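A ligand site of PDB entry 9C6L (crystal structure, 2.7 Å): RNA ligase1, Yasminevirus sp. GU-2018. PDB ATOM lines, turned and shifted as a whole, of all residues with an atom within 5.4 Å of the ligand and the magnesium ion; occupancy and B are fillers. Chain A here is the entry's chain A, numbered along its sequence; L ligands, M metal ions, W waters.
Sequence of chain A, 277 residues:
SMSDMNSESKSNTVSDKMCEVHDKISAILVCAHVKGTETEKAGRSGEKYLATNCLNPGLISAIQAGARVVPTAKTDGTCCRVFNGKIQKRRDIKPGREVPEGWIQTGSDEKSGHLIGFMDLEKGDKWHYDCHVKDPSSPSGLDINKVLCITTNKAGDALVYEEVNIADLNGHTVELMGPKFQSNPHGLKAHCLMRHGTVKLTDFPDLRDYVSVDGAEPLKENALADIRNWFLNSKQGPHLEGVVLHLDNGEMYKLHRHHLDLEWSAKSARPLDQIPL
No residue comes within 4 Å of the magnesium ion.
The nearest printed residue that does not touch the magnesium ion is Lys 74 (4.9 Å).
The side-chain amino group (NZ) of Lys 254 lies within salt-bridge range of an oxygen (O2) of the ligand, at 3.2 Å.
N2 of the ligand lies within hydrogen-bond range of N of Thr 75, 3.3 Å away.
NE2 of His 196 sits at hydrogen-bond distance from O7 of the ligand, at 3.3 Å.
A nitrogen (N4) of the ligand sits at hydrogen-bond distance from a ring nitrogen (NE2) of His 246, at 3.1 Å.
The side-chain amino group (NZ) of Lys 74 is in salt-bridge range of an oxygen (O1) of the ligand (3.996 Å).
The backbone carbonyl oxygen (O) of Ala 73 lies within hydrogen-bond range of a nitrogen (N3) of the ligand, at 3.1 Å.
The side-chain carboxylate of Glu 175 lies within hydrogen-bond range of an oxygen (O7) of the ligand (2.5 Å).
OG1 of Thr 72 is in hydrogen-bond range of N3 of the ligand, 3.5 Å away.
An oxygen (O6) of the ligand sits at hydrogen-bond distance from the guanidinium group (NH1) of Arg 90 (3.5 Å).
O7 of the ligand lies close to SG of Cys 79 (3.5 Å).
The magnesium ion is bound by O3 of the ligand (2.0 Å), water W2 (2.3 Å) and water W1 (2.4 Å).
The magnesium ion has three donor atoms within binding distance.
Water W2 bridges OD1 of Asp 76 (3.3 Å) and O of Gly 77 (3.4 Å).
The side-chain carboxylate (OE1) of Glu 175 lies within hydrogen-bond range of a ring nitrogen (NE2) of His 196 (3.0 Å).
The backbone NH of Arg 90 sits at hydrogen-bond distance from the backbone carbonyl oxygen of Cys 79 (3.2 Å).
The side-chain amino group of Lys 74 lies within salt-bridge range of the side-chain carboxylate of Glu 241 (2.8 Å).
NE2 of His 246 lies close to SD of Met 252.
The backbone carbonyl oxygen (O) of Val 244 sits at hydrogen-bond distance from the side-chain hydroxyl (OG1) of Thr 72, at 2.5 Å.
N of Gly 77 sits at hydrogen-bond distance from OE2 of Glu 175 (3.0 Å).
O of Val 174 sits close to NE2 of His 196 (3.5 Å).
The side-chain amino group (NZ) of Lys 254 lies within hydrogen-bond range of the backbone carbonyl oxygen (O) of Ile 25, at 2.9 Å.
A nitrogen (N3) of the ligand lies close to the backbone NH (N) of Gly 197.
Residues that only touch the ligand: Val 244 and Ile 25.
Of the 23 residues printed, 13 come within 4 Å of the ligand.
The nearest printed residue that does not touch the ligand is Met 252 (4.1 Å).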
ATOM      1  N   VAL A  21      15.619  17.236 -20.479  1.00  0.00           N
ATOM      2  CA  VAL A  21      16.452  18.090 -19.624  1.00  0.00           C
ATOM      3  C   VAL A  21      17.011  17.210 -18.507  1.00  0.00           C
ATOM      4  O   VAL A  21      16.315  16.896 -17.534  1.00  0.00           O
ATOM      5  CB  VAL A  21      15.689  19.301 -19.086  1.00  0.00           C
ATOM      6  CG1 VAL A  21      14.346  18.896 -18.495  1.00  0.00           C
ATOM      7  CG2 VAL A  21      16.530  20.050 -18.058  1.00  0.00           C
ATOM      8  N   ILE A  25      21.787  23.308 -18.913  1.00  0.00           N
ATOM      9  CA  ILE A  25      21.797  23.699 -20.313  1.00  0.00           C
ATOM     10  C   ILE A  25      22.744  24.869 -20.509  1.00  0.00           C
ATOM     11  O   ILE A  25      22.781  25.810 -19.700  1.00  0.00           O
ATOM     12  CB  ILE A  25      20.379  24.041 -20.793  1.00  0.00           C
ATOM     13  CG1 ILE A  25      19.423  22.889 -20.459  1.00  0.00           C
ATOM     14  CG2 ILE A  25      20.375  24.311 -22.292  1.00  0.00           C
ATOM     15  CD1 ILE A  25      18.005  23.090 -20.975  1.00  0.00           C
ATOM     16  N   THR A  72      12.734  26.216 -29.587  1.00  0.00           N
ATOM     17  CA  THR A  72      11.556  25.964 -28.781  1.00  0.00           C
ATOM     18  C   THR A  72      11.315  27.141 -27.841  1.00  0.00           C
ATOM     19  O   THR A  72      12.122  28.066 -27.744  1.00  0.00           O
ATOM     20  CB  THR A  72      11.696  24.658 -27.980  1.00  0.00           C
ATOM     21  OG1 THR A  72      12.687  24.828 -26.952  1.00  0.00           O
ATOM     22  CG2 THR A  72      12.092  23.512 -28.898  1.00  0.00           C
ATOM     23  N   ALA A  73      10.190  27.092 -27.136  1.00  0.00           N
ATOM     24  CA  ALA A  73       9.765  28.177 -26.263  1.00  0.00           C
ATOM     25  C   ALA A  73      10.122  27.846 -24.826  1.00  0.00           C
ATOM     26  O   ALA A  73       9.652  26.843 -24.274  1.00  0.00           O
ATOM     27  CB  ALA A  73       8.257  28.412 -26.384  1.00  0.00           C
ATOM     28  N   LYS A  74      10.948  28.686 -24.211  1.00  0.00           N
ATOM     29  CA  LYS A  74      11.300  28.518 -22.807  1.00  0.00           C
ATOM     30  C   LYS A  74      10.168  29.060 -21.934  1.00  0.00           C
ATOM     31  O   LYS A  74       9.741  30.203 -22.098  1.00  0.00           O
ATOM     32  CB  LYS A  74      12.612  29.234 -22.483  1.00  0.00           C
ATOM     33  CG  LYS A  74      13.274  28.759 -21.197  1.00  0.00           C
ATOM     34  CD  LYS A  74      14.404  29.683 -20.784  1.00  0.00           C
ATOM     35  CE  LYS A  74      15.231  29.087 -19.645  1.00  0.00           C
ATOM     36  NZ  LYS A  74      14.388  28.756 -18.455  1.00  0.00           N
ATOM     37  N   THR A  75       9.686  28.232 -21.017  1.00  0.00           N
ATOM     38  CA  THR A  75       8.616  28.604 -20.104  1.00  0.00           C
ATOM     39  C   THR A  75       9.157  28.594 -18.681  1.00  0.00           C
ATOM     40  O   THR A  75      10.187  27.985 -18.390  1.00  0.00           O
ATOM     41  CB  THR A  75       7.409  27.663 -20.241  1.00  0.00           C
ATOM     42  OG1 THR A  75       6.287  28.211 -19.534  1.00  0.00           O
ATOM     43  CG2 THR A  75       7.725  26.284 -19.697  1.00  0.00           C
ATOM     44  N   ASP A  76       8.474  29.303 -17.782  1.00  0.00           N
ATOM     45  CA  ASP A  76       8.965  29.555 -16.436  1.00  0.00           C
ATOM     46  C   ASP A  76       8.169  28.718 -15.449  1.00  0.00           C
ATOM     47  O   ASP A  76       6.978  28.964 -15.228  1.00  0.00           O
ATOM     48  CB  ASP A  76       8.884  31.028 -16.082  1.00  0.00           C
ATOM     49  CG  ASP A  76       9.631  31.371 -14.804  1.00  0.00           C
ATOM     50  OD1 ASP A  76      10.281  30.463 -14.242  1.00  0.00           O
ATOM     51  OD2 ASP A  76       9.558  32.543 -14.366  1.00  0.00           O
ATOM     52  N   GLY A  77       8.816  27.728 -14.852  1.00  0.00           N
ATOM     53  CA  GLY A  77       8.209  26.917 -13.832  1.00  0.00           C
ATOM     54  C   GLY A  77       9.266  26.130 -13.092  1.00  0.00           C
ATOM     55  O   GLY A  77      10.417  26.572 -12.994  1.00  0.00           O
ATOM     56  N   THR A  78       8.887  24.973 -12.575  1.00  0.00           N
ATOM     57  CA  THR A  78       9.797  24.065 -11.909  1.00  0.00           C
ATOM     58  C   THR A  78      10.005  22.833 -12.785  1.00  0.00           C
ATOM     59  O   THR A  78       9.042  22.282 -13.340  1.00  0.00           O
ATOM     60  CB  THR A  78       9.271  23.638 -10.538  1.00  0.00           C
ATOM     61  OG1 THR A  78      10.188  22.720  -9.929  1.00  0.00           O
ATOM     62  CG2 THR A  78       7.907  22.982 -10.643  1.00  0.00           C
ATOM     63  N   CYS A  79      11.261  22.415 -12.913  1.00  0.00           N
ATOM     64  CA  CYS A  79      11.580  21.269 -13.766  1.00  0.00           C
ATOM     65  C   CYS A  79      11.089  19.986 -13.133  1.00  0.00           C
ATOM     66  O   CYS A  79      11.343  19.718 -11.949  1.00  0.00           O
ATOM     67  CB  CYS A  79      13.084  21.199 -14.003  1.00  0.00           C
ATOM     68  SG  CYS A  79      13.579  19.849 -15.099  1.00  0.00           S
ATOM     69  N   ARG A  90      12.690  17.731  -9.859  1.00  0.00           N
ATOM     70  CA  ARG A  90      14.139  17.836  -9.931  1.00  0.00           C
ATOM     71  C   ARG A  90      14.694  18.367  -8.613  1.00  0.00           C
ATOM     72  O   ARG A  90      14.124  19.280  -7.999  1.00  0.00           O
ATOM     73  CB  ARG A  90      14.541  18.759 -11.085  1.00  0.00           C
ATOM     74  CG  ARG A  90      16.005  19.179 -11.062  1.00  0.00           C
ATOM     75  CD  ARG A  90      16.389  19.911 -12.329  1.00  0.00           C
ATOM     76  NE  ARG A  90      17.658  20.625 -12.176  1.00  0.00           N
ATOM     77  CZ  ARG A  90      18.257  21.310 -13.141  1.00  0.00           C
ATOM     78  NH1 ARG A  90      17.744  21.377 -14.358  1.00  0.00           N
ATOM     79  NH2 ARG A  90      19.401  21.939 -12.881  1.00  0.00           N
ATOM     80  N   VAL A 174       8.975  17.664 -18.230  1.00  0.00           N
ATOM     81  CA  VAL A 174       7.958  18.699 -18.348  1.00  0.00           C
ATOM     82  C   VAL A 174       8.315  19.858 -17.428  1.00  0.00           C
ATOM     83  O   VAL A 174       9.079  19.700 -16.472  1.00  0.00           O
ATOM     84  CB  VAL A 174       6.541  18.166 -18.001  1.00  0.00           C
ATOM     85  CG1 VAL A 174       6.097  17.129 -19.016  1.00  0.00           C
ATOM     86  CG2 VAL A 174       6.529  17.582 -16.597  1.00  0.00           C
ATOM     87  N   GLU A 175       7.760  21.020 -17.737  1.00  0.00           N
ATOM     88  CA  GLU A 175       7.850  22.189 -16.863  1.00  0.00           C
ATOM     89  C   GLU A 175       6.510  22.343 -16.162  1.00  0.00           C
ATOM     90  O   GLU A 175       5.481  22.605 -16.806  1.00  0.00           O
ATOM     91  CB  GLU A 175       8.201  23.441 -17.647  1.00  0.00           C
ATOM     92  CG  GLU A 175       8.628  24.610 -16.765  1.00  0.00           C
ATOM     93  CD  GLU A 175      10.072  24.542 -16.329  1.00  0.00           C
ATOM     94  OE1 GLU A 175      10.740  23.527 -16.653  1.00  0.00           O
ATOM     95  OE2 GLU A 175      10.550  25.485 -15.673  1.00  0.00           O
ATOM     96  N   ARG A 195       5.206  19.580 -21.877  1.00  0.00           N
ATOM     97  CA  ARG A 195       6.366  18.876 -22.411  1.00  0.00           C
ATOM     98  C   ARG A 195       7.383  19.865 -22.966  1.00  0.00           C
ATOM     99  O   ARG A 195       7.048  20.730 -23.781  1.00  0.00           O
ATOM    100  CB  ARG A 195       5.920  17.897 -23.503  1.00  0.00           C
ATOM    101  CG  ARG A 195       7.050  17.276 -24.324  1.00  0.00           C
ATOM    102  CD  ARG A 195       7.868  16.274 -23.527  1.00  0.00           C
ATOM    103  NE  ARG A 195       8.965  15.726 -24.316  1.00  0.00           N
ATOM    104  CZ  ARG A 195      10.254  16.009 -24.145  1.00  0.00           C
ATOM    105  NH1 ARG A 195      10.662  16.808 -23.157  1.00  0.00           N
ATOM    106  NH2 ARG A 195      11.150  15.478 -24.959  1.00  0.00           N
ATOM    107  N   HIS A 196       8.632  19.735 -22.510  1.00  0.00           N
ATOM    108  CA  HIS A 196       9.696  20.585 -23.007  1.00  0.00           C
ATOM    109  C   HIS A 196       9.844  20.415 -24.517  1.00  0.00           C
ATOM    110  O   HIS A 196       9.949  19.298 -25.021  1.00  0.00           O
ATOM    111  CB  HIS A 196      11.011  20.250 -22.315  1.00  0.00           C
ATOM    112  CG  HIS A 196      11.021  20.585 -20.857  1.00  0.00           C
ATOM    113  ND1 HIS A 196      11.521  19.734 -19.893  1.00  0.00           N
ATOM    114  CD2 HIS A 196      10.588  21.686 -20.188  1.00  0.00           C
ATOM    115  CE1 HIS A 196      11.400  20.292 -18.703  1.00  0.00           C
ATOM    116  NE2 HIS A 196      10.836  21.476 -18.857  1.00  0.00           N
ATOM    117  N   GLY A 197       9.842  21.544 -25.232  1.00  0.00           N
ATOM    118  CA  GLY A 197       9.949  21.535 -26.675  1.00  0.00           C
ATOM    119  C   GLY A 197       8.627  21.566 -27.416  1.00  0.00           C
ATOM    120  O   GLY A 197       8.628  21.578 -28.650  1.00  0.00           O
ATOM    121  N   THR A 198       7.500  21.596 -26.686  1.00  0.00           N
ATOM    122  CA  THR A 198       6.192  21.560 -27.337  1.00  0.00           C
ATOM    123  C   THR A 198       6.019  22.722 -28.298  1.00  0.00           C
ATOM    124  O   THR A 198       5.662  22.534 -29.464  1.00  0.00           O
ATOM    125  CB  THR A 198       5.098  21.577 -26.274  1.00  0.00           C
ATOM    126  OG1 THR A 198       5.104  20.331 -25.554  1.00  0.00           O
ATOM    127  CG2 THR A 198       3.724  21.787 -26.910  1.00  0.00           C
ATOM    128  N   GLU A 241       9.538  33.212 -21.580  1.00  0.00           N
ATOM    129  CA  GLU A 241      10.656  33.528 -20.695  1.00  0.00           C
ATOM    130  C   GLU A 241      11.969  33.586 -21.452  1.00  0.00           C
ATOM    131  O   GLU A 241      12.850  34.393 -21.113  1.00  0.00           O
ATOM    132  CB  GLU A 241      10.736  32.486 -19.576  1.00  0.00           C
ATOM    133  CG  GLU A 241      11.909  32.667 -18.623  1.00  0.00           C
ATOM    134  CD  GLU A 241      12.129  31.450 -17.740  1.00  0.00           C
ATOM    135  OE1 GLU A 241      12.091  30.313 -18.267  1.00  0.00           O
ATOM    136  OE2 GLU A 241      12.328  31.630 -16.517  1.00  0.00           O
ATOM    137  N   VAL A 244      14.975  27.905 -26.090  1.00  0.00           N
ATOM    138  CA  VAL A 244      15.825  26.727 -25.911  1.00  0.00           C
ATOM    139  C   VAL A 244      15.931  26.011 -27.238  1.00  0.00           C
ATOM    140  O   VAL A 244      14.917  25.564 -27.797  1.00  0.00           O
ATOM    141  CB  VAL A 244      15.281  25.786 -24.811  1.00  0.00           C
ATOM    142  CG1 VAL A 244      16.233  24.608 -24.615  1.00  0.00           C
ATOM    143  CG2 VAL A 244      15.070  26.543 -23.514  1.00  0.00           C
ATOM    144  N   HIS A 246      16.723  22.882 -29.447  1.00  0.00           N
ATOM    145  CA  HIS A 246      16.767  21.430 -29.357  1.00  0.00           C
ATOM    146  C   HIS A 246      17.387  20.879 -30.642  1.00  0.00           C
ATOM    147  O   HIS A 246      16.857  21.094 -31.729  1.00  0.00           O
ATOM    148  CB  HIS A 246      15.365  20.852 -29.142  1.00  0.00           C
ATOM    149  CG  HIS A 246      14.845  21.033 -27.748  1.00  0.00           C
ATOM    150  ND1 HIS A 246      14.453  19.980 -26.957  1.00  0.00           N
ATOM    151  CD2 HIS A 246      14.656  22.154 -27.008  1.00  0.00           C
ATOM    152  CE1 HIS A 246      14.032  20.433 -25.790  1.00  0.00           C
ATOM    153  NE2 HIS A 246      14.152  21.751 -25.801  1.00  0.00           N
ATOM    154  N   MET A 252      21.233  20.929 -26.029  1.00  0.00           N
ATOM    155  CA  MET A 252      20.328  22.060 -25.927  1.00  0.00           C
ATOM    156  C   MET A 252      21.117  23.309 -25.566  1.00  0.00           C
ATOM    157  O   MET A 252      22.179  23.247 -24.934  1.00  0.00           O
ATOM    158  CB  MET A 252      19.238  21.822 -24.877  1.00  0.00           C
ATOM    159  CG  MET A 252      18.170  20.826 -25.317  1.00  0.00           C
ATOM    160  SD  MET A 252      16.905  20.547 -24.057  1.00  0.00           S
ATOM    161  CE  MET A 252      17.883  19.750 -22.784  1.00  0.00           C
ATOM    162  N   LYS A 254      20.178  27.478 -24.317  1.00  0.00           N
ATOM    163  CA  LYS A 254      19.101  28.315 -23.823  1.00  0.00           C
ATOM    164  C   LYS A 254      19.518  29.787 -23.792  1.00  0.00           C
ATOM    165  O   LYS A 254      20.710  30.119 -23.772  1.00  0.00           O
ATOM    166  CB  LYS A 254      18.662  27.890 -22.406  1.00  0.00           C
ATOM    167  CG  LYS A 254      19.765  27.967 -21.360  1.00  0.00           C
ATOM    168  CD  LYS A 254      19.185  27.987 -19.950  1.00  0.00           C
ATOM    169  CE  LYS A 254      20.261  28.125 -18.899  1.00  0.00           C
ATOM    170  NZ  LYS A 254      20.500  26.846 -18.162  1.00  0.00           N
ATOM    171  N   HIS A 256      17.711  32.993 -21.536  1.00  0.00           N
ATOM    172  CA  HIS A 256      16.694  33.645 -20.746  1.00  0.00           C
ATOM    173  C   HIS A 256      16.618  35.122 -21.118  1.00  0.00           C
ATOM    174  O   HIS A 256      17.549  35.694 -21.674  1.00  0.00           O
ATOM    175  CB  HIS A 256      17.015  33.488 -19.249  1.00  0.00           C
ATOM    176  CG  HIS A 256      15.856  33.775 -18.347  1.00  0.00           C
ATOM    177  ND1 HIS A 256      15.437  35.052 -18.044  1.00  0.00           N
ATOM    178  CD2 HIS A 256      15.037  32.940 -17.650  1.00  0.00           C
ATOM    179  CE1 HIS A 256      14.409  35.001 -17.216  1.00  0.00           C
ATOM    180  NE2 HIS A 256      14.144  33.731 -16.960  1.00  0.00           N
HETATM  181  P1  LIG L   1      17.357  27.903 -16.142  1.00  0.00           P
HETATM  182  O1  LIG L   1      17.816  29.304 -16.475  1.00  0.00           O
HETATM  183  O2  LIG L   1      18.468  27.004 -15.657  1.00  0.00           O
HETATM  184  O3  LIG L   1      16.107  27.847 -15.305  1.00  0.00           O
HETATM  185  O4  LIG L   1      16.927  27.304 -17.553  1.00  0.00           O
HETATM  186  C1  LIG L   1      16.798  25.890 -17.746  1.00  0.00           C
HETATM  187  C2  LIG L   1      15.439  25.399 -17.302  1.00  0.00           C
HETATM  188  O5  LIG L   1      14.445  25.760 -18.279  1.00  0.00           O
HETATM  189  C3  LIG L   1      15.346  23.885 -17.150  1.00  0.00           C
HETATM  190  O6  LIG L   1      15.396  23.522 -15.768  1.00  0.00           O
HETATM  191  C4  LIG L   1      13.978  23.503 -17.777  1.00  0.00           C
HETATM  192  O7  LIG L   1      13.107  22.800 -16.917  1.00  0.00           O
HETATM  193  C5  LIG L   1      13.384  24.846 -18.211  1.00  0.00           C
HETATM  194  N1  LIG L   1      12.687  24.817 -19.512  1.00  0.00           N
HETATM  195  C6  LIG L   1      11.532  25.469 -19.728  1.00  0.00           C
HETATM  196  N2  LIG L   1      11.084  25.282 -20.993  1.00  0.00           N
HETATM  197  C7  LIG L   1      11.968  24.495 -21.614  1.00  0.00           C
HETATM  198  C8  LIG L   1      12.082  23.910 -22.963  1.00  0.00           C
HETATM  199  N3  LIG L   1      11.158  24.152 -23.916  1.00  0.00           N
HETATM  200  N4  LIG L   1      13.157  23.130 -23.209  1.00  0.00           N
HETATM  201  C9  LIG L   1      14.087  22.879 -22.265  1.00  0.00           C
HETATM  202  N5  LIG L   1      14.034  23.376 -21.029  1.00  0.00           N
HETATM  203  C10 LIG L   1      13.024  24.173 -20.633  1.00  0.00           C
HETATM  204 MG    MG M   1      15.057  28.065 -13.671  1.00  0.00          MG
HETATM  205  O   HOH W   1      17.135  28.723 -12.636  1.00  0.00           O
HETATM  206  O   HOH W   2      12.958  28.874 -13.167  1.00  0.00           O
